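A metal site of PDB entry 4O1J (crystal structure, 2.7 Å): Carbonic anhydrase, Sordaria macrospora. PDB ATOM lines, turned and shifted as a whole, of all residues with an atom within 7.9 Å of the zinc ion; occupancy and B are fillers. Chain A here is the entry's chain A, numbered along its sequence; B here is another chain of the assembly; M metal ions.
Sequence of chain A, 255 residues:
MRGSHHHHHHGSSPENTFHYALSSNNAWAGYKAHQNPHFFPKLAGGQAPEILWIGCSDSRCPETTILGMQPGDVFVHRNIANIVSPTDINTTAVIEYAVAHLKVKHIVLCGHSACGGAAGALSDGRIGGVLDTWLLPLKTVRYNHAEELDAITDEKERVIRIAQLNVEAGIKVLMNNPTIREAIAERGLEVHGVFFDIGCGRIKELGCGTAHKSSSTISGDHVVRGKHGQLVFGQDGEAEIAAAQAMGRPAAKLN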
ATOM      1  N   GLY A  55       7.149  11.681  24.478  1.00  0.00           N
ATOM      2  CA  GLY A  55       6.164  12.293  23.615  1.00  0.00           C
ATOM      3  C   GLY A  55       6.669  12.949  22.351  1.00  0.00           C
ATOM      4  O   GLY A  55       7.870  12.960  22.029  1.00  0.00           O
ATOM      5  N   CYS A  56       5.712  13.526  21.612  1.00  0.00           N
ATOM      6  CA  CYS A  56       6.023  14.213  20.373  1.00  0.00           C
ATOM      7  C   CYS A  56       6.519  15.614  20.671  1.00  0.00           C
ATOM      8  O   CYS A  56       6.032  16.272  21.580  1.00  0.00           O
ATOM      9  CB  CYS A  56       4.790  14.255  19.453  1.00  0.00           C
ATOM     10  SG  CYS A  56       5.160  14.846  17.773  1.00  0.00           S
ATOM     11  N   SER A  57       7.465  16.072  19.859  1.00  0.00           N
ATOM     12  CA  SER A  57       8.083  17.380  19.987  1.00  0.00           C
ATOM     13  C   SER A  57       7.079  18.522  19.810  1.00  0.00           C
ATOM     14  O   SER A  57       7.380  19.671  20.157  1.00  0.00           O
ATOM     15  CB  SER A  57       9.203  17.527  18.945  1.00  0.00           C
ATOM     16  OG  SER A  57      10.367  16.837  19.354  1.00  0.00           O
ATOM     17  N   ASP A  58       5.909  18.182  19.278  1.00  0.00           N
ATOM     18  CA  ASP A  58       4.790  19.094  19.016  1.00  0.00           C
ATOM     19  C   ASP A  58       4.656  20.181  20.087  1.00  0.00           C
ATOM     20  O   ASP A  58       4.700  19.886  21.288  1.00  0.00           O
ATOM     21  CB  ASP A  58       3.489  18.287  18.931  1.00  0.00           C
ATOM     22  CG  ASP A  58       2.394  19.002  18.166  1.00  0.00           C
ATOM     23  OD1 ASP A  58       1.804  19.954  18.718  1.00  0.00           O
ATOM     24  OD2 ASP A  58       2.116  18.598  17.007  1.00  0.00           O
ATOM     25  N   SER A  59       4.508  21.421  19.643  1.00  0.00           N
ATOM     26  CA  SER A  59       4.449  22.551  20.568  1.00  0.00           C
ATOM     27  C   SER A  59       3.192  22.496  21.429  1.00  0.00           C
ATOM     28  O   SER A  59       3.127  23.099  22.504  1.00  0.00           O
ATOM     29  CB  SER A  59       4.519  23.889  19.802  1.00  0.00           C
ATOM     30  OG  SER A  59       3.481  24.008  18.852  1.00  0.00           O
ATOM     31  N   ARG A  60       2.201  21.750  20.960  1.00  0.00           N
ATOM     32  CA  ARG A  60       0.931  21.692  21.644  1.00  0.00           C
ATOM     33  C   ARG A  60       0.894  20.582  22.701  1.00  0.00           C
ATOM     34  O   ARG A  60      -0.131  20.351  23.348  1.00  0.00           O
ATOM     35  CB  ARG A  60      -0.187  21.486  20.620  1.00  0.00           C
ATOM     36  CG  ARG A  60      -0.134  22.514  19.502  1.00  0.00           C
ATOM     37  CD  ARG A  60      -1.055  22.121  18.363  1.00  0.00           C
ATOM     38  NE  ARG A  60      -0.513  21.022  17.581  1.00  0.00           N
ATOM     39  CZ  ARG A  60      -1.164  20.413  16.592  1.00  0.00           C
ATOM     40  NH1 ARG A  60      -2.392  20.785  16.268  1.00  0.00           N
ATOM     41  NH2 ARG A  60      -0.579  19.413  15.938  1.00  0.00           N
ATOM     42  N   CYS A  61       2.024  19.913  22.920  1.00  0.00           N
ATOM     43  CA  CYS A  61       2.058  18.800  23.858  1.00  0.00           C
ATOM     44  C   CYS A  61       3.081  18.917  25.000  1.00  0.00           C
ATOM     45  O   CYS A  61       3.841  17.969  25.210  1.00  0.00           O
ATOM     46  CB  CYS A  61       2.338  17.509  23.097  1.00  0.00           C
ATOM     47  SG  CYS A  61       1.122  17.095  21.833  1.00  0.00           S
ATOM     48  N   ASN A  79      10.547  13.621  20.826  1.00  0.00           N
ATOM     49  CA  ASN A  79      11.081  13.650  19.472  1.00  0.00           C
ATOM     50  C   ASN A  79       9.961  13.748  18.452  1.00  0.00           C
ATOM     51  O   ASN A  79       8.781  13.876  18.814  1.00  0.00           O
ATOM     52  CB  ASN A  79      11.943  12.413  19.200  1.00  0.00           C
ATOM     53  CG  ASN A  79      11.177  11.116  19.375  1.00  0.00           C
ATOM     54  OD1 ASN A  79      10.183  10.853  18.701  1.00  0.00           O
ATOM     55  ND2 ASN A  79      11.675  10.274  20.269  1.00  0.00           N
ATOM     56  N   ILE A  80      10.311  13.700  17.176  1.00  0.00           N
ATOM     57  CA  ILE A  80       9.314  13.752  16.123  1.00  0.00           C
ATOM     58  C   ILE A  80       8.386  12.534  16.160  1.00  0.00           C
ATOM     59  O   ILE A  80       8.841  11.404  16.036  1.00  0.00           O
ATOM     60  CB  ILE A  80       9.959  13.855  14.741  1.00  0.00           C
ATOM     61  CG1 ILE A  80      10.725  15.172  14.636  1.00  0.00           C
ATOM     62  CG2 ILE A  80       8.901  13.780  13.644  1.00  0.00           C
ATOM     63  CD1 ILE A  80       9.879  16.412  14.905  1.00  0.00           C
ATOM     64  N   ALA A  81       7.097  12.789  16.394  1.00  0.00           N
ATOM     65  CA  ALA A  81       6.044  11.771  16.351  1.00  0.00           C
ATOM     66  C   ALA A  81       6.188  10.720  17.440  1.00  0.00           C
ATOM     67  O   ALA A  81       5.698   9.605  17.287  1.00  0.00           O
ATOM     68  CB  ALA A  81       6.002  11.112  14.974  1.00  0.00           C
ATOM     69  N   ASN A  82       6.853  11.097  18.546  1.00  0.00           N
ATOM     70  CA  ASN A  82       7.102  10.224  19.710  1.00  0.00           C
ATOM     71  C   ASN A  82       7.454   8.790  19.370  1.00  0.00           C
ATOM     72  O   ASN A  82       6.841   7.846  19.875  1.00  0.00           O
ATOM     73  CB  ASN A  82       5.891  10.226  20.673  1.00  0.00           C
ATOM     74  CG  ASN A  82       4.564   9.968  19.969  1.00  0.00           C
ATOM     75  OD1 ASN A  82       3.912  10.903  19.486  1.00  0.00           O
ATOM     76  ND2 ASN A  82       4.148   8.706  19.927  1.00  0.00           N
ATOM     77  N   CYS A 110       3.150   8.769  24.993  1.00  0.00           N
ATOM     78  CA  CYS A 110       1.983   9.551  24.630  1.00  0.00           C
ATOM     79  C   CYS A 110       1.970   9.948  23.171  1.00  0.00           C
ATOM     80  O   CYS A 110       2.810  10.720  22.737  1.00  0.00           O
ATOM     81  CB  CYS A 110       1.897  10.807  25.501  1.00  0.00           C
ATOM     82  SG  CYS A 110       0.459  11.845  25.113  1.00  0.00           S
ATOM     83  N   GLY A 111       0.965   9.460  22.448  1.00  0.00           N
ATOM     84  CA  GLY A 111       0.748   9.927  21.090  1.00  0.00           C
ATOM     85  C   GLY A 111      -0.348  10.972  21.117  1.00  0.00           C
ATOM     86  O   GLY A 111      -0.994  11.132  22.142  1.00  0.00           O
ATOM     87  N   HIS A 112      -0.539  11.682  20.009  1.00  0.00           N
ATOM     88  CA  HIS A 112      -1.551  12.732  19.961  1.00  0.00           C
ATOM     89  C   HIS A 112      -2.166  12.923  18.578  1.00  0.00           C
ATOM     90  O   HIS A 112      -1.639  12.441  17.579  1.00  0.00           O
ATOM     91  CB  HIS A 112      -0.967  14.065  20.429  1.00  0.00           C
ATOM     92  CG  HIS A 112      -0.073  14.707  19.417  1.00  0.00           C
ATOM     93  ND1 HIS A 112      -0.539  15.608  18.478  1.00  0.00           N
ATOM     94  CD2 HIS A 112       1.262  14.591  19.197  1.00  0.00           C
ATOM     95  CE1 HIS A 112       0.466  16.012  17.716  1.00  0.00           C
ATOM     96  NE2 HIS A 112       1.563  15.416  18.134  1.00  0.00           N
ATOM     97  N   SER A 113      -3.284  13.647  18.556  1.00  0.00           N
ATOM     98  CA  SER A 113      -3.990  13.973  17.333  1.00  0.00           C
ATOM     99  C   SER A 113      -3.325  15.123  16.572  1.00  0.00           C
ATOM    100  O   SER A 113      -2.632  15.955  17.165  1.00  0.00           O
ATOM    101  CB  SER A 113      -5.447  14.313  17.655  1.00  0.00           C
ATOM    102  OG  SER A 113      -5.528  15.297  18.674  1.00  0.00           O
ATOM    103  N   ALA A 114      -3.552  15.175  15.259  1.00  0.00           N
ATOM    104  CA  ALA A 114      -2.962  16.176  14.369  1.00  0.00           C
ATOM    105  C   ALA A 114      -1.433  16.114  14.404  1.00  0.00           C
ATOM    106  O   ALA A 114      -0.756  17.143  14.360  1.00  0.00           O
ATOM    107  CB  ALA A 114      -3.447  17.574  14.726  1.00  0.00           C
ATOM    108  N   CYS A 115      -0.903  14.892  14.482  1.00  0.00           N
ATOM    109  CA  CYS A 115       0.538  14.690  14.475  1.00  0.00           C
ATOM    110  C   CYS A 115       1.078  14.846  13.047  1.00  0.00           C
ATOM    111  O   CYS A 115       0.657  14.138  12.127  1.00  0.00           O
ATOM    112  CB  CYS A 115       0.883  13.314  15.028  1.00  0.00           C
ATOM    113  SG  CYS A 115       2.628  13.069  15.412  1.00  0.00           S
ATOM    114  N   GLY A 116       2.027  15.761  12.896  1.00  0.00           N
ATOM    115  CA  GLY A 116       2.612  16.044  11.604  1.00  0.00           C
ATOM    116  C   GLY A 116       3.434  14.894  11.064  1.00  0.00           C
ATOM    117  O   GLY A 116       3.448  14.653   9.858  1.00  0.00           O
ATOM    118  N   GLY A 117       4.111  14.182  11.964  1.00  0.00           N
ATOM    119  CA  GLY A 117       4.930  13.048  11.571  1.00  0.00           C
ATOM    120  C   GLY A 117       4.058  11.916  11.078  1.00  0.00           C
ATOM    121  O   GLY A 117       4.393  11.235  10.114  1.00  0.00           O
ATOM    122  N   ALA A 118       2.920  11.733  11.748  1.00  0.00           N
ATOM    123  CA  ALA A 118       1.921  10.746  11.346  1.00  0.00           C
ATOM    124  C   ALA A 118       1.403  11.015   9.934  1.00  0.00           C
ATOM    125  O   ALA A 118       1.358  10.130   9.074  1.00  0.00           O
ATOM    126  CB  ALA A 118       0.776  10.732  12.346  1.00  0.00           C
ATOM    127  N   ALA A 119       0.980  12.264   9.707  1.00  0.00           N
ATOM    128  CA  ALA A 119       0.518  12.708   8.393  1.00  0.00           C
ATOM    129  C   ALA A 119       1.606  12.532   7.330  1.00  0.00           C
ATOM    130  O   ALA A 119       1.316  12.146   6.194  1.00  0.00           O
ATOM    131  CB  ALA A 119       0.074  14.160   8.461  1.00  0.00           C
ATOM    132  N   ALA A 163      -1.465   7.436  14.316  1.00  0.00           N
ATOM    133  CA  ALA A 163      -0.728   7.897  15.506  1.00  0.00           C
ATOM    134  C   ALA A 163      -0.913   6.948  16.706  1.00  0.00           C
ATOM    135  O   ALA A 163       0.030   6.692  17.472  1.00  0.00           O
ATOM    136  CB  ALA A 163      -1.139   9.296  15.872  1.00  0.00           C
ATOM    137  N   ILE A 198      -6.056  16.692  21.210  1.00  0.00           N
ATOM    138  CA  ILE A 198      -5.895  18.136  21.341  1.00  0.00           C
ATOM    139  C   ILE A 198      -7.217  18.891  21.296  1.00  0.00           C
ATOM    140  O   ILE A 198      -7.396  19.887  22.006  1.00  0.00           O
ATOM    141  CB  ILE A 198      -4.945  18.676  20.260  1.00  0.00           C
ATOM    142  CG1 ILE A 198      -3.598  17.961  20.346  1.00  0.00           C
ATOM    143  CG2 ILE A 198      -4.751  20.178  20.404  1.00  0.00           C
ATOM    144  CD1 ILE A 198      -2.567  18.470  19.390  1.00  0.00           C
ATOM    145  N   GLN B  47      -0.328  24.416  14.423  1.00  0.00           N
ATOM    146  CA  GLN B  47       0.618  25.052  15.328  1.00  0.00           C
ATOM    147  C   GLN B  47       1.506  26.024  14.584  1.00  0.00           C
ATOM    148  O   GLN B  47       1.809  25.841  13.399  1.00  0.00           O
ATOM    149  CB  GLN B  47       1.469  24.005  16.062  1.00  0.00           C
ATOM    150  CG  GLN B  47       2.428  23.234  15.158  1.00  0.00           C
ATOM    151  CD  GLN B  47       3.180  22.138  15.889  1.00  0.00           C
ATOM    152  OE1 GLN B  47       3.727  22.362  16.972  1.00  0.00           O
ATOM    153  NE2 GLN B  47       3.199  20.954  15.311  1.00  0.00           N
ATOM    154  N   PHE B  75       8.204  24.355  20.373  1.00  0.00           N
ATOM    155  CA  PHE B  75       8.493  23.039  19.799  1.00  0.00           C
ATOM    156  C   PHE B  75       9.749  22.475  20.453  1.00  0.00           C
ATOM    157  O   PHE B  75      10.779  23.136  20.426  1.00  0.00           O
ATOM    158  CB  PHE B  75       8.689  23.191  18.282  1.00  0.00           C
ATOM    159  CG  PHE B  75       8.573  21.920  17.496  1.00  0.00           C
ATOM    160  CD1 PHE B  75       7.339  21.303  17.319  1.00  0.00           C
ATOM    161  CD2 PHE B  75       9.691  21.360  16.898  1.00  0.00           C
ATOM    162  CE1 PHE B  75       7.229  20.134  16.581  1.00  0.00           C
ATOM    163  CE2 PHE B  75       9.591  20.193  16.149  1.00  0.00           C
ATOM    164  CZ  PHE B  75       8.355  19.575  15.990  1.00  0.00           C
ATOM    165  N   TYR B  97      12.548  19.397  11.140  1.00  0.00           N
ATOM    166  CA  TYR B  97      11.110  19.658  11.104  1.00  0.00           C
ATOM    167  C   TYR B  97      10.796  21.058  11.616  1.00  0.00           C
ATOM    168  O   TYR B  97       9.943  21.759  11.067  1.00  0.00           O
ATOM    169  CB  TYR B  97      10.348  18.617  11.918  1.00  0.00           C
ATOM    170  CG  TYR B  97       8.873  18.562  11.568  1.00  0.00           C
ATOM    171  CD1 TYR B  97       8.433  17.760  10.524  1.00  0.00           C
ATOM    172  CD2 TYR B  97       7.932  19.322  12.264  1.00  0.00           C
ATOM    173  CE1 TYR B  97       7.082  17.702  10.190  1.00  0.00           C
ATOM    174  CE2 TYR B  97       6.592  19.273  11.932  1.00  0.00           C
ATOM    175  CZ  TYR B  97       6.168  18.453  10.888  1.00  0.00           C
ATOM    176  OH  TYR B  97       4.840  18.392  10.545  1.00  0.00           O
HETATM  177 ZN    ZN M   1       3.218  15.002  16.614  1.00  0.00          ZN
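The side-chain sulfur (SG) of Cys 56 sits close to the backbone NH (N) of Ala 81, 3.1 Å away.
The guanidinium group (NE) of Arg 60 lies within salt-bridge range of the side-chain carboxylate (OD1) of Asp 58 (2.8 Å).
The side-chain carboxylate (OD2) of Asp 58 lies close to a ring nitrogen (NE2) of His 112, at 3.4 Å.
N of Asp 58 lies close to SG of Cys 56, 3.7 Å away.
OD2 of Asp 58 lies within hydrogen-bond range of NE2 of Gln 47 of chain B, at 3.1 Å.
OD2 of Asp 58 touches the zinc ion, 3.8 Å away.
Gly 116 touches the zinc ion (N to ZN, 3.98 Å).
Five residues have an atom within 4 Å of the zinc ion: Cys 56, Asp 58, His 112, Cys 115 and Gly 116.
The nearest printed residue that does not touch the zinc ion is Ala 81 (4.3 Å).
The zinc ion is bound by the side-chain sulfur of Cys 56 (2.3 Å), a ring nitrogen (NE2) of His 112 (2.3 Å) and the side-chain sulfur of Cys 115 (2.4 Å).
The zinc ion has three donor atoms within binding distance.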
